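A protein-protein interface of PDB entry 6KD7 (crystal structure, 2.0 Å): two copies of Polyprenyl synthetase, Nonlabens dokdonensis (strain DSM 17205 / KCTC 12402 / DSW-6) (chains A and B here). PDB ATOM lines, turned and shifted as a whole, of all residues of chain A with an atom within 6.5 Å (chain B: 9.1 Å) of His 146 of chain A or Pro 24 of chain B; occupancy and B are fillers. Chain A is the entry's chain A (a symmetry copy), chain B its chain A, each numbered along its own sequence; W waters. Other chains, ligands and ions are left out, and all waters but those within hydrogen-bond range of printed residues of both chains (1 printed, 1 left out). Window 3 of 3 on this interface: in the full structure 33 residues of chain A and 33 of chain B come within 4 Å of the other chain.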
ATOM      1  N   GLU A 139     -23.515 -16.507  32.374  1.00  0.00           N
ATOM      2  CA  GLU A 139     -24.881 -16.653  31.834  1.00  0.00           C
ATOM      3  C   GLU A 139     -24.824 -16.588  30.300  1.00  0.00           C
ATOM      4  O   GLU A 139     -25.579 -17.312  29.643  1.00  0.00           O
ATOM      5  CB  GLU A 139     -25.778 -15.535  32.384  1.00  0.00           C
ATOM      6  CG  GLU A 139     -26.269 -15.827  33.793  1.00  0.00           C
ATOM      7  CD  GLU A 139     -26.907 -14.646  34.518  1.00  0.00           C
ATOM      8  OE1 GLU A 139     -26.625 -13.473  34.156  1.00  0.00           O
ATOM      9  OE2 GLU A 139     -27.646 -14.929  35.442  1.00  0.00           O
ATOM     10  N   CYS A 141     -22.381 -17.535  28.422  1.00  0.00           N
ATOM     11  CA  CYS A 141     -21.890 -18.886  27.993  1.00  0.00           C
ATOM     12  C   CYS A 141     -23.066 -19.881  27.955  1.00  0.00           C
ATOM     13  O   CYS A 141     -23.221 -20.637  26.952  1.00  0.00           O
ATOM     14  CB  CYS A 141     -20.760 -19.403  28.868  1.00  0.00           C
ATOM     15  SG  CYS A 141     -19.262 -18.397  28.759  1.00  0.00           S
ATOM     16  N   GLU A 142     -23.920 -19.868  28.971  1.00  0.00           N
ATOM     17  CA  GLU A 142     -25.059 -20.795  29.049  1.00  0.00           C
ATOM     18  C   GLU A 142     -26.014 -20.483  27.909  1.00  0.00           C
ATOM     19  O   GLU A 142     -26.540 -21.419  27.307  1.00  0.00           O
ATOM     20  CB  GLU A 142     -25.779 -20.720  30.389  1.00  0.00           C
ATOM     21  CG  GLU A 142     -24.894 -21.149  31.542  1.00  0.00           C
ATOM     22  CD  GLU A 142     -25.553 -21.088  32.920  1.00  0.00           C
ATOM     23  OE1 GLU A 142     -26.728 -20.661  32.963  1.00  0.00           O
ATOM     24  OE2 GLU A 142     -24.884 -21.474  33.927  1.00  0.00           O
ATOM     25  N   GLY A 143     -26.282 -19.213  27.653  1.00  0.00           N
ATOM     26  CA  GLY A 143     -27.199 -18.869  26.560  1.00  0.00           C
ATOM     27  C   GLY A 143     -26.686 -19.388  25.212  1.00  0.00           C
ATOM     28  O   GLY A 143     -27.509 -19.828  24.423  1.00  0.00           O
ATOM     29  N   GLN A 144     -25.378 -19.282  24.972  1.00  0.00           N
ATOM     30  CA  GLN A 144     -24.707 -19.759  23.751  1.00  0.00           C
ATOM     31  C   GLN A 144     -24.957 -21.258  23.658  1.00  0.00           C
ATOM     32  O   GLN A 144     -25.372 -21.730  22.557  1.00  0.00           O
ATOM     33  CB  GLN A 144     -23.198 -19.528  23.754  1.00  0.00           C
ATOM     34  CG  GLN A 144     -22.779 -18.093  23.447  1.00  0.00           C
ATOM     35  CD  GLN A 144     -23.199 -17.640  22.062  1.00  0.00           C
ATOM     36  OE1 GLN A 144     -23.552 -18.462  21.189  1.00  0.00           O
ATOM     37  NE2 GLN A 144     -23.171 -16.319  21.861  1.00  0.00           N
ATOM     38  N   GLN A 145     -24.741 -21.978  24.755  1.00  0.00           N
ATOM     39  CA  GLN A 145     -24.886 -23.452  24.700  1.00  0.00           C
ATOM     40  C   GLN A 145     -26.332 -23.822  24.424  1.00  0.00           C
ATOM     41  O   GLN A 145     -26.539 -24.760  23.675  1.00  0.00           O
ATOM     42  CB  GLN A 145     -24.444 -24.145  25.972  1.00  0.00           C
ATOM     43  CG  GLN A 145     -24.469 -25.666  25.859  1.00  0.00           C
ATOM     44  CD  GLN A 145     -23.590 -26.187  24.747  1.00  0.00           C
ATOM     45  OE1 GLN A 145     -22.438 -25.773  24.592  1.00  0.00           O
ATOM     46  NE2 GLN A 145     -24.180 -27.043  23.928  1.00  0.00           N
ATOM     47  N   HIS A 146     -27.298 -23.131  25.026  1.00  0.00           N
ATOM     48  CA  HIS A 146     -28.726 -23.419  24.781  1.00  0.00           C
ATOM     49  C   HIS A 146     -28.996 -23.221  23.289  1.00  0.00           C
ATOM     50  O   HIS A 146     -29.721 -24.022  22.705  1.00  0.00           O
ATOM     51  CB  HIS A 146     -29.641 -22.517  25.629  1.00  0.00           C
ATOM     52  CG  HIS A 146     -29.667 -22.901  27.069  1.00  0.00           C
ATOM     53  ND1 HIS A 146     -29.403 -22.006  28.102  1.00  0.00           N
ATOM     54  CD2 HIS A 146     -29.904 -24.072  27.657  1.00  0.00           C
ATOM     55  CE1 HIS A 146     -29.470 -22.630  29.254  1.00  0.00           C
ATOM     56  NE2 HIS A 146     -29.770 -23.888  29.000  1.00  0.00           N
ATOM     57  N   ASP A 147     -28.497 -22.141  22.711  1.00  0.00           N
ATOM     58  CA  ASP A 147     -28.779 -21.828  21.294  1.00  0.00           C
ATOM     59  C   ASP A 147     -28.208 -22.978  20.424  1.00  0.00           C
ATOM     60  O   ASP A 147     -28.869 -23.395  19.468  1.00  0.00           O
ATOM     61  CB  ASP A 147     -28.180 -20.489  20.911  1.00  0.00           C
ATOM     62  CG  ASP A 147     -28.821 -19.856  19.684  1.00  0.00           C
ATOM     63  OD1 ASP A 147     -29.959 -20.140  19.377  1.00  0.00           O
ATOM     64  OD2 ASP A 147     -28.180 -19.067  19.087  1.00  0.00           O
ATOM     65  N   VAL A 148     -27.042 -23.497  20.770  1.00  0.00           N
ATOM     66  CA  VAL A 148     -26.405 -24.647  20.063  1.00  0.00           C
ATOM     67  C   VAL A 148     -27.308 -25.868  20.253  1.00  0.00           C
ATOM     68  O   VAL A 148     -27.581 -26.516  19.259  1.00  0.00           O
ATOM     69  CB  VAL A 148     -24.970 -24.922  20.557  1.00  0.00           C
ATOM     70  CG1 VAL A 148     -24.421 -26.257  20.045  1.00  0.00           C
ATOM     71  CG2 VAL A 148     -24.069 -23.795  20.137  1.00  0.00           C
ATOM     72  N   ASP A 149     -27.737 -26.146  21.485  1.00  0.00           N
ATOM     73  CA  ASP A 149     -28.591 -27.320  21.773  1.00  0.00           C
ATOM     74  C   ASP A 149     -29.880 -27.233  20.932  1.00  0.00           C
ATOM     75  O   ASP A 149     -30.372 -28.284  20.485  1.00  0.00           O
ATOM     76  CB  ASP A 149     -28.880 -27.451  23.261  1.00  0.00           C
ATOM     77  CG  ASP A 149     -27.655 -27.732  24.123  1.00  0.00           C
ATOM     78  OD1 ASP A 149     -26.597 -28.134  23.572  1.00  0.00           O
ATOM     79  OD2 ASP A 149     -27.747 -27.481  25.328  1.00  0.00           O
ATOM     80  N   PHE A 150     -30.437 -26.044  20.713  1.00  0.00           N
ATOM     81  CA  PHE A 150     -31.717 -25.916  19.982  1.00  0.00           C
ATOM     82  C   PHE A 150     -31.553 -26.354  18.514  1.00  0.00           C
ATOM     83  O   PHE A 150     -32.548 -26.745  17.891  1.00  0.00           O
ATOM     84  CB  PHE A 150     -32.240 -24.476  20.001  1.00  0.00           C
ATOM     85  CG  PHE A 150     -32.725 -23.939  21.322  1.00  0.00           C
ATOM     86  CD1 PHE A 150     -32.927 -24.759  22.420  1.00  0.00           C
ATOM     87  CD2 PHE A 150     -32.981 -22.585  21.452  1.00  0.00           C
ATOM     88  CE1 PHE A 150     -33.365 -24.244  23.627  1.00  0.00           C
ATOM     89  CE2 PHE A 150     -33.447 -22.070  22.658  1.00  0.00           C
ATOM     90  CZ  PHE A 150     -33.630 -22.901  23.742  1.00  0.00           C
ATOM     91  N   GLU A 151     -30.329 -26.325  18.007  1.00  0.00           N
ATOM     92  CA  GLU A 151     -30.080 -26.692  16.594  1.00  0.00           C
ATOM     93  C   GLU A 151     -30.518 -28.134  16.333  1.00  0.00           C
ATOM     94  O   GLU A 151     -30.883 -28.415  15.210  1.00  0.00           O
ATOM     95  CB  GLU A 151     -28.606 -26.547  16.229  1.00  0.00           C
ATOM     96  CG  GLU A 151     -28.117 -25.121  16.220  1.00  0.00           C
ATOM     97  CD  GLU A 151     -26.626 -25.000  15.978  1.00  0.00           C
ATOM     98  OE1 GLU A 151     -26.003 -26.009  15.680  1.00  0.00           O
ATOM     99  OE2 GLU A 151     -26.106 -23.891  16.094  1.00  0.00           O
ATOM    100  N   GLU A 160     -38.658 -21.558  26.492  1.00  0.00           N
ATOM    101  CA  GLU A 160     -37.230 -21.974  26.415  1.00  0.00           C
ATOM    102  C   GLU A 160     -36.471 -21.005  25.505  1.00  0.00           C
ATOM    103  O   GLU A 160     -35.400 -20.613  25.871  1.00  0.00           O
ATOM    104  CB  GLU A 160     -37.096 -23.378  25.850  1.00  0.00           C
ATOM    105  CG  GLU A 160     -37.514 -24.477  26.811  1.00  0.00           C
ATOM    106  CD  GLU A 160     -37.486 -25.822  26.093  1.00  0.00           C
ATOM    107  OE1 GLU A 160     -38.104 -25.944  25.026  1.00  0.00           O
ATOM    108  OE2 GLU A 160     -36.734 -26.675  26.531  1.00  0.00           O
ATOM    109  N   ASN A 163     -35.953 -17.660  27.470  1.00  0.00           N
ATOM    110  CA  ASN A 163     -34.884 -17.914  28.465  1.00  0.00           C
ATOM    111  C   ASN A 163     -33.522 -17.884  27.754  1.00  0.00           C
ATOM    112  O   ASN A 163     -32.573 -17.262  28.284  1.00  0.00           O
ATOM    113  CB  ASN A 163     -35.163 -19.208  29.231  1.00  0.00           C
ATOM    114  CG  ASN A 163     -34.101 -19.436  30.277  1.00  0.00           C
ATOM    115  OD1 ASN A 163     -33.979 -18.618  31.158  1.00  0.00           O
ATOM    116  ND2 ASN A 163     -33.243 -20.430  30.106  1.00  0.00           N
ATOM    117  N   MET A 164     -33.415 -18.476  26.556  1.00  0.00           N
ATOM    118  CA  MET A 164     -32.108 -18.535  25.877  1.00  0.00           C
ATOM    119  C   MET A 164     -31.681 -17.111  25.475  1.00  0.00           C
ATOM    120  O   MET A 164     -30.517 -16.706  25.788  1.00  0.00           O
ATOM    121  CB  MET A 164     -32.173 -19.488  24.685  1.00  0.00           C
ATOM    122  CG  MET A 164     -30.883 -19.535  23.868  1.00  0.00           C
ATOM    123  SD  MET A 164     -30.703 -18.209  22.660  1.00  0.00           S
ATOM    124  CE  MET A 164     -31.974 -18.652  21.471  1.00  0.00           C
ATOM    125  N   LEU A 167     -30.484 -14.958  28.464  1.00  0.00           N
ATOM    126  CA  LEU A 167     -29.077 -15.275  28.855  1.00  0.00           C
ATOM    127  C   LEU A 167     -28.096 -14.803  27.777  1.00  0.00           C
ATOM    128  O   LEU A 167     -27.025 -14.264  28.110  1.00  0.00           O
ATOM    129  CB  LEU A 167     -28.958 -16.782  29.103  1.00  0.00           C
ATOM    130  CG  LEU A 167     -29.764 -17.301  30.290  1.00  0.00           C
ATOM    131  CD1 LEU A 167     -29.799 -18.809  30.356  1.00  0.00           C
ATOM    132  CD2 LEU A 167     -29.168 -16.784  31.581  1.00  0.00           C
ATOM    133  N   ALA B  21     -21.722 -27.049  38.885  1.00  0.00           N
ATOM    134  CA  ALA B  21     -22.628 -26.699  37.770  1.00  0.00           C
ATOM    135  C   ALA B  21     -22.797 -27.926  36.872  1.00  0.00           C
ATOM    136  O   ALA B  21     -21.793 -28.537  36.558  1.00  0.00           O
ATOM    137  CB  ALA B  21     -22.045 -25.549  37.000  1.00  0.00           C
ATOM    138  N   THR B  22     -24.031 -28.283  36.522  1.00  0.00           N
ATOM    139  CA  THR B  22     -24.231 -29.453  35.635  1.00  0.00           C
ATOM    140  C   THR B  22     -25.067 -29.116  34.395  1.00  0.00           C
ATOM    141  O   THR B  22     -24.937 -29.827  33.413  1.00  0.00           O
ATOM    142  CB  THR B  22     -24.832 -30.633  36.402  1.00  0.00           C
ATOM    143  OG1 THR B  22     -26.129 -30.226  36.817  1.00  0.00           O
ATOM    144  CG2 THR B  22     -24.009 -31.020  37.606  1.00  0.00           C
ATOM    145  N   GLU B  23     -25.906 -28.085  34.458  1.00  0.00           N
ATOM    146  CA  GLU B  23     -26.807 -27.771  33.319  1.00  0.00           C
ATOM    147  C   GLU B  23     -26.511 -26.377  32.762  1.00  0.00           C
ATOM    148  O   GLU B  23     -26.391 -25.469  33.567  1.00  0.00           O
ATOM    149  CB  GLU B  23     -28.264 -27.918  33.743  1.00  0.00           C
ATOM    150  CG  GLU B  23     -28.689 -29.357  33.915  1.00  0.00           C
ATOM    151  CD  GLU B  23     -30.028 -29.509  34.610  1.00  0.00           C
ATOM    152  OE1 GLU B  23     -30.585 -30.621  34.579  1.00  0.00           O
ATOM    153  OE2 GLU B  23     -30.509 -28.516  35.184  1.00  0.00           O
ATOM    154  N   PRO B  24     -26.430 -26.167  31.429  1.00  0.00           N
ATOM    155  CA  PRO B  24     -26.598 -27.219  30.419  1.00  0.00           C
ATOM    156  C   PRO B  24     -25.390 -28.159  30.285  1.00  0.00           C
ATOM    157  O   PRO B  24     -24.297 -27.696  30.308  1.00  0.00           O
ATOM    158  CB  PRO B  24     -26.830 -26.437  29.126  1.00  0.00           C
ATOM    159  CG  PRO B  24     -26.043 -25.185  29.330  1.00  0.00           C
ATOM    160  CD  PRO B  24     -26.167 -24.881  30.804  1.00  0.00           C
ATOM    161  N   ALA B  25     -25.663 -29.443  30.081  1.00  0.00           N
ATOM    162  CA  ALA B  25     -24.629 -30.496  30.027  1.00  0.00           C
ATOM    163  C   ALA B  25     -23.618 -30.203  28.918  1.00  0.00           C
ATOM    164  O   ALA B  25     -22.453 -30.435  29.156  1.00  0.00           O
ATOM    165  CB  ALA B  25     -25.286 -31.834  29.831  1.00  0.00           C
ATOM    166  N   GLY B  26     -24.070 -29.694  27.775  1.00  0.00           N
ATOM    167  CA  GLY B  26     -23.172 -29.367  26.642  1.00  0.00           C
ATOM    168  C   GLY B  26     -22.071 -28.382  27.026  1.00  0.00           C
ATOM    169  O   GLY B  26     -20.993 -28.338  26.353  1.00  0.00           O
ATOM    170  N   LEU B  27     -22.329 -27.563  28.047  1.00  0.00           N
ATOM    171  CA  LEU B  27     -21.310 -26.621  28.543  1.00  0.00           C
ATOM    172  C   LEU B  27     -20.473 -27.260  29.667  1.00  0.00           C
ATOM    173  O   LEU B  27     -19.234 -27.069  29.675  1.00  0.00           O
ATOM    174  CB  LEU B  27     -22.042 -25.380  29.042  1.00  0.00           C
ATOM    175  CG  LEU B  27     -21.096 -24.280  29.474  1.00  0.00           C
ATOM    176  CD1 LEU B  27     -20.307 -23.770  28.264  1.00  0.00           C
ATOM    177  CD2 LEU B  27     -21.858 -23.143  30.153  1.00  0.00           C
ATOM    178  N   TYR B  28     -21.108 -27.903  30.654  1.00  0.00           N
ATOM    179  CA  TYR B  28     -20.431 -28.242  31.942  1.00  0.00           C
ATOM    180  C   TYR B  28     -19.905 -29.687  31.944  1.00  0.00           C
ATOM    181  O   TYR B  28     -18.892 -29.913  32.638  1.00  0.00           O
ATOM    182  CB  TYR B  28     -21.346 -27.955  33.136  1.00  0.00           C
ATOM    183  CG  TYR B  28     -21.629 -26.486  33.349  1.00  0.00           C
ATOM    184  CD1 TYR B  28     -20.620 -25.607  33.723  1.00  0.00           C
ATOM    185  CD2 TYR B  28     -22.908 -25.970  33.211  1.00  0.00           C
ATOM    186  CE1 TYR B  28     -20.868 -24.263  33.963  1.00  0.00           C
ATOM    187  CE2 TYR B  28     -23.164 -24.620  33.432  1.00  0.00           C
ATOM    188  CZ  TYR B  28     -22.152 -23.776  33.841  1.00  0.00           C
ATOM    189  OH  TYR B  28     -22.417 -22.455  34.023  1.00  0.00           O
ATOM    190  N   ASP B  29     -20.455 -30.608  31.149  1.00  0.00           N
ATOM    191  CA  ASP B  29     -19.925 -32.010  31.121  1.00  0.00           C
ATOM    192  C   ASP B  29     -18.422 -32.011  30.857  1.00  0.00           C
ATOM    193  O   ASP B  29     -17.669 -32.647  31.582  1.00  0.00           O
ATOM    194  CB  ASP B  29     -20.550 -32.885  30.037  1.00  0.00           C
ATOM    195  CG  ASP B  29     -21.933 -33.398  30.353  1.00  0.00           C
ATOM    196  OD1 ASP B  29     -22.406 -33.196  31.514  1.00  0.00           O
ATOM    197  OD2 ASP B  29     -22.530 -33.988  29.413  1.00  0.00           O
ATOM    198  N   PRO B  30     -17.905 -31.224  29.883  1.00  0.00           N
ATOM    199  CA  PRO B  30     -16.480 -31.178  29.646  1.00  0.00           C
ATOM    200  C   PRO B  30     -15.684 -30.575  30.800  1.00  0.00           C
ATOM    201  O   PRO B  30     -14.498 -30.859  30.899  1.00  0.00           O
ATOM    202  CB  PRO B  30     -16.321 -30.360  28.352  1.00  0.00           C
ATOM    203  CG  PRO B  30     -17.684 -30.288  27.762  1.00  0.00           C
ATOM    204  CD  PRO B  30     -18.628 -30.347  28.953  1.00  0.00           C
ATOM    205  N   VAL B  31     -16.298 -29.777  31.670  1.00  0.00           N
ATOM    206  CA  VAL B  31     -15.531 -29.234  32.822  1.00  0.00           C
ATOM    207  C   VAL B  31     -15.238 -30.403  33.773  1.00  0.00           C
ATOM    208  O   VAL B  31     -14.090 -30.551  34.210  1.00  0.00           O
ATOM    209  CB  VAL B  31     -16.303 -28.132  33.549  1.00  0.00           C
ATOM    210  CG1 VAL B  31     -15.537 -27.669  34.790  1.00  0.00           C
ATOM    211  CG2 VAL B  31     -16.636 -26.971  32.619  1.00  0.00           C
ATOM    212  N   HIS B  32     -16.246 -31.186  34.114  1.00  0.00           N
ATOM    213  CA  HIS B  32     -16.068 -32.368  35.012  1.00  0.00           C
ATOM    214  C   HIS B  32     -15.062 -33.364  34.390  1.00  0.00           C
ATOM    215  O   HIS B  32     -14.166 -33.874  35.100  1.00  0.00           O
ATOM    216  CB  HIS B  32     -17.423 -32.986  35.331  1.00  0.00           C
ATOM    217  CG  HIS B  32     -18.301 -32.026  36.063  1.00  0.00           C
ATOM    218  ND1 HIS B  32     -19.482 -31.517  35.511  1.00  0.00           N
ATOM    219  CD2 HIS B  32     -18.136 -31.388  37.234  1.00  0.00           C
ATOM    220  CE1 HIS B  32     -20.011 -30.661  36.354  1.00  0.00           C
ATOM    221  NE2 HIS B  32     -19.209 -30.558  37.395  1.00  0.00           N
ATOM    222  N   TRP B  98     -15.823 -34.126  22.181  1.00  0.00           N
ATOM    223  CA  TRP B  98     -17.007 -33.324  21.807  1.00  0.00           C
ATOM    224  C   TRP B  98     -16.697 -32.699  20.451  1.00  0.00           C
ATOM    225  O   TRP B  98     -16.751 -33.408  19.463  1.00  0.00           O
ATOM    226  CB  TRP B  98     -17.298 -32.266  22.875  1.00  0.00           C
ATOM    227  CG  TRP B  98     -18.002 -32.814  24.076  1.00  0.00           C
ATOM    228  CD1 TRP B  98     -19.344 -32.968  24.240  1.00  0.00           C
ATOM    229  CD2 TRP B  98     -17.398 -33.301  25.283  1.00  0.00           C
ATOM    230  NE1 TRP B  98     -19.615 -33.509  25.461  1.00  0.00           N
ATOM    231  CE2 TRP B  98     -18.443 -33.732  26.120  1.00  0.00           C
ATOM    232  CE3 TRP B  98     -16.082 -33.424  25.735  1.00  0.00           C
ATOM    233  CZ2 TRP B  98     -18.210 -34.263  27.381  1.00  0.00           C
ATOM    234  CZ3 TRP B  98     -15.855 -33.958  26.978  1.00  0.00           C
ATOM    235  CH2 TRP B  98     -16.905 -34.364  27.791  1.00  0.00           C
ATOM    236  N   THR B 102     -17.183 -26.691  21.429  1.00  0.00           N
ATOM    237  CA  THR B 102     -17.347 -27.081  22.837  1.00  0.00           C
ATOM    238  C   THR B 102     -16.071 -26.700  23.563  1.00  0.00           C
ATOM    239  O   THR B 102     -16.130 -26.169  24.651  1.00  0.00           O
ATOM    240  CB  THR B 102     -17.699 -28.564  22.970  1.00  0.00           C
ATOM    241  OG1 THR B 102     -18.964 -28.772  22.331  1.00  0.00           O
ATOM    242  CG2 THR B 102     -17.730 -29.007  24.409  1.00  0.00           C
ATOM    243  N   LEU B 105     -15.965 -22.723  23.983  1.00  0.00           N
ATOM    244  CA  LEU B 105     -17.000 -22.161  24.875  1.00  0.00           C
ATOM    245  C   LEU B 105     -16.812 -22.692  26.294  1.00  0.00           C
ATOM    246  O   LEU B 105     -16.895 -21.877  27.230  1.00  0.00           O
ATOM    247  CB  LEU B 105     -18.373 -22.546  24.340  1.00  0.00           C
ATOM    248  CG  LEU B 105     -19.531 -21.985  25.148  1.00  0.00           C
ATOM    249  CD1 LEU B 105     -19.501 -20.451  25.084  1.00  0.00           C
ATOM    250  CD2 LEU B 105     -20.834 -22.507  24.601  1.00  0.00           C
ATOM    251  N   THR B 106     -16.592 -24.005  26.472  1.00  0.00           N
ATOM    252  CA  THR B 106     -16.384 -24.567  27.827  1.00  0.00           C
ATOM    253  C   THR B 106     -15.137 -23.937  28.429  1.00  0.00           C
ATOM    254  O   THR B 106     -15.129 -23.667  29.644  1.00  0.00           O
ATOM    255  CB  THR B 106     -16.336 -26.093  27.808  1.00  0.00           C
ATOM    256  OG1 THR B 106     -17.668 -26.444  27.442  1.00  0.00           O
ATOM    257  CG2 THR B 106     -15.987 -26.677  29.142  1.00  0.00           C
ATOM    258  N   ALA B 109     -16.076 -20.611  29.822  1.00  0.00           N
ATOM    259  CA  ALA B 109     -16.909 -20.782  31.032  1.00  0.00           C
ATOM    260  C   ALA B 109     -15.975 -21.116  32.211  1.00  0.00           C
ATOM    261  O   ALA B 109     -16.178 -20.550  33.299  1.00  0.00           O
ATOM    262  CB  ALA B 109     -17.989 -21.785  30.851  1.00  0.00           C
HETATM  263  O   HOH W   1     -26.660 -29.233  26.994  1.00  0.00           O
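The backbone carbonyl oxygen of Gly 26 of chain B sits close to the side-chain amide oxygen of Gln 145 of chain A (3.4 Å).
OH of Tyr 28 of chain B lies within hydrogen-bond range of OE2 of Glu 142 of chain A (2.7 Å).
The backbone carbonyl oxygen of Leu 27 of chain B is in hydrogen-bond range of the side-chain hydroxyl of Thr 106 of chain B, at 2.8 Å.
The backbone carbonyl oxygen of Tyr 28 of chain B lies within hydrogen-bond range of a ring nitrogen (ND1) of His 32 of chain B, at 3.3 Å.
A ring nitrogen (ND1) of His 146 of chain A sits at hydrogen-bond distance from the backbone carbonyl oxygen (O) of Glu 142 of chain A (3.0 Å).
The side-chain carboxylate of Asp 149 of chain A lies within hydrogen-bond range of the side-chain amide nitrogen of Gln 145 of chain A, 2.7 Å away.
Cys 141 of chain A touches Leu 105 of chain B (O to CD2, 3.8 Å).
Leu 27 of chain B touches Glu 142 of chain A (CD2 to CG, 3.9 Å).
Gln 144 of chain A touches Leu 105 of chain B (CB to CD2, 3.9 Å).
Gln 145 of chain A touches Pro 24 of chain B.
Gln 145 of chain A touches Leu 27 of chain B (CG to N, 3.6 Å).
OE1 of Gln 145 of chain A touches CD2 of Leu 105 of chain B (3.6 Å).
Pro 24 of chain B touches His 146 of chain A (CB to NE2, 3.9 Å).
His 146 of chain A touches just one residue of chain B: Pro 24 (3.9 Å).
Of the printed residues of chain A, Pro 24 of chain B touches Gln 145 (3.8 Å) and His 146 (3.9 Å).
Of the printed residues of chain A, Leu 105 of chain B touches Cys 141 (3.8 Å), Gln 144 (3.9 Å) and Gln 145 (3.6 Å).
Of the printed residues of chain B, Gln 145 of chain A touches Pro 24, Gly 26, Leu 27 and Leu 105.
Printed residues of chain A within 4 Å of Leu 27 of chain B: Glu 142 and Gln 145.
Printed residues of chain B within 4 Å of Glu 142 of chain A: Leu 27 (3.9 Å) and Tyr 28 (2.7 Å).
Met 164 of chain A touches none of the printed residues of chain B.
Thr 22 of chain B touches none of the printed residues of chain A.
The nearest printed residue of chain A that does not touch Pro 24 of chain B is Glu 142 of chain A (4.01 Å).
Of the 17 printed residues of chain B, 5 touch a printed residue of chain A.
Hydrophobic or aromatic side chains of chain B that line the printed part of chain A: Pro 24, Leu 27, Tyr 28 and Leu 105.
No position is printed for both chains.
Of the 9 pairs that touch across the chains among the printed residues, none has its exchanged pair printed and touching as well.
Water W1 lies within hydrogen-bond range of the side-chain carboxylate of Asp 149 of chain A (2.7 Å), the backbone NH of Gly 26 of chain B (2.7 Å) and the backbone NH of Ala 25 of chain B (3.3 Å).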
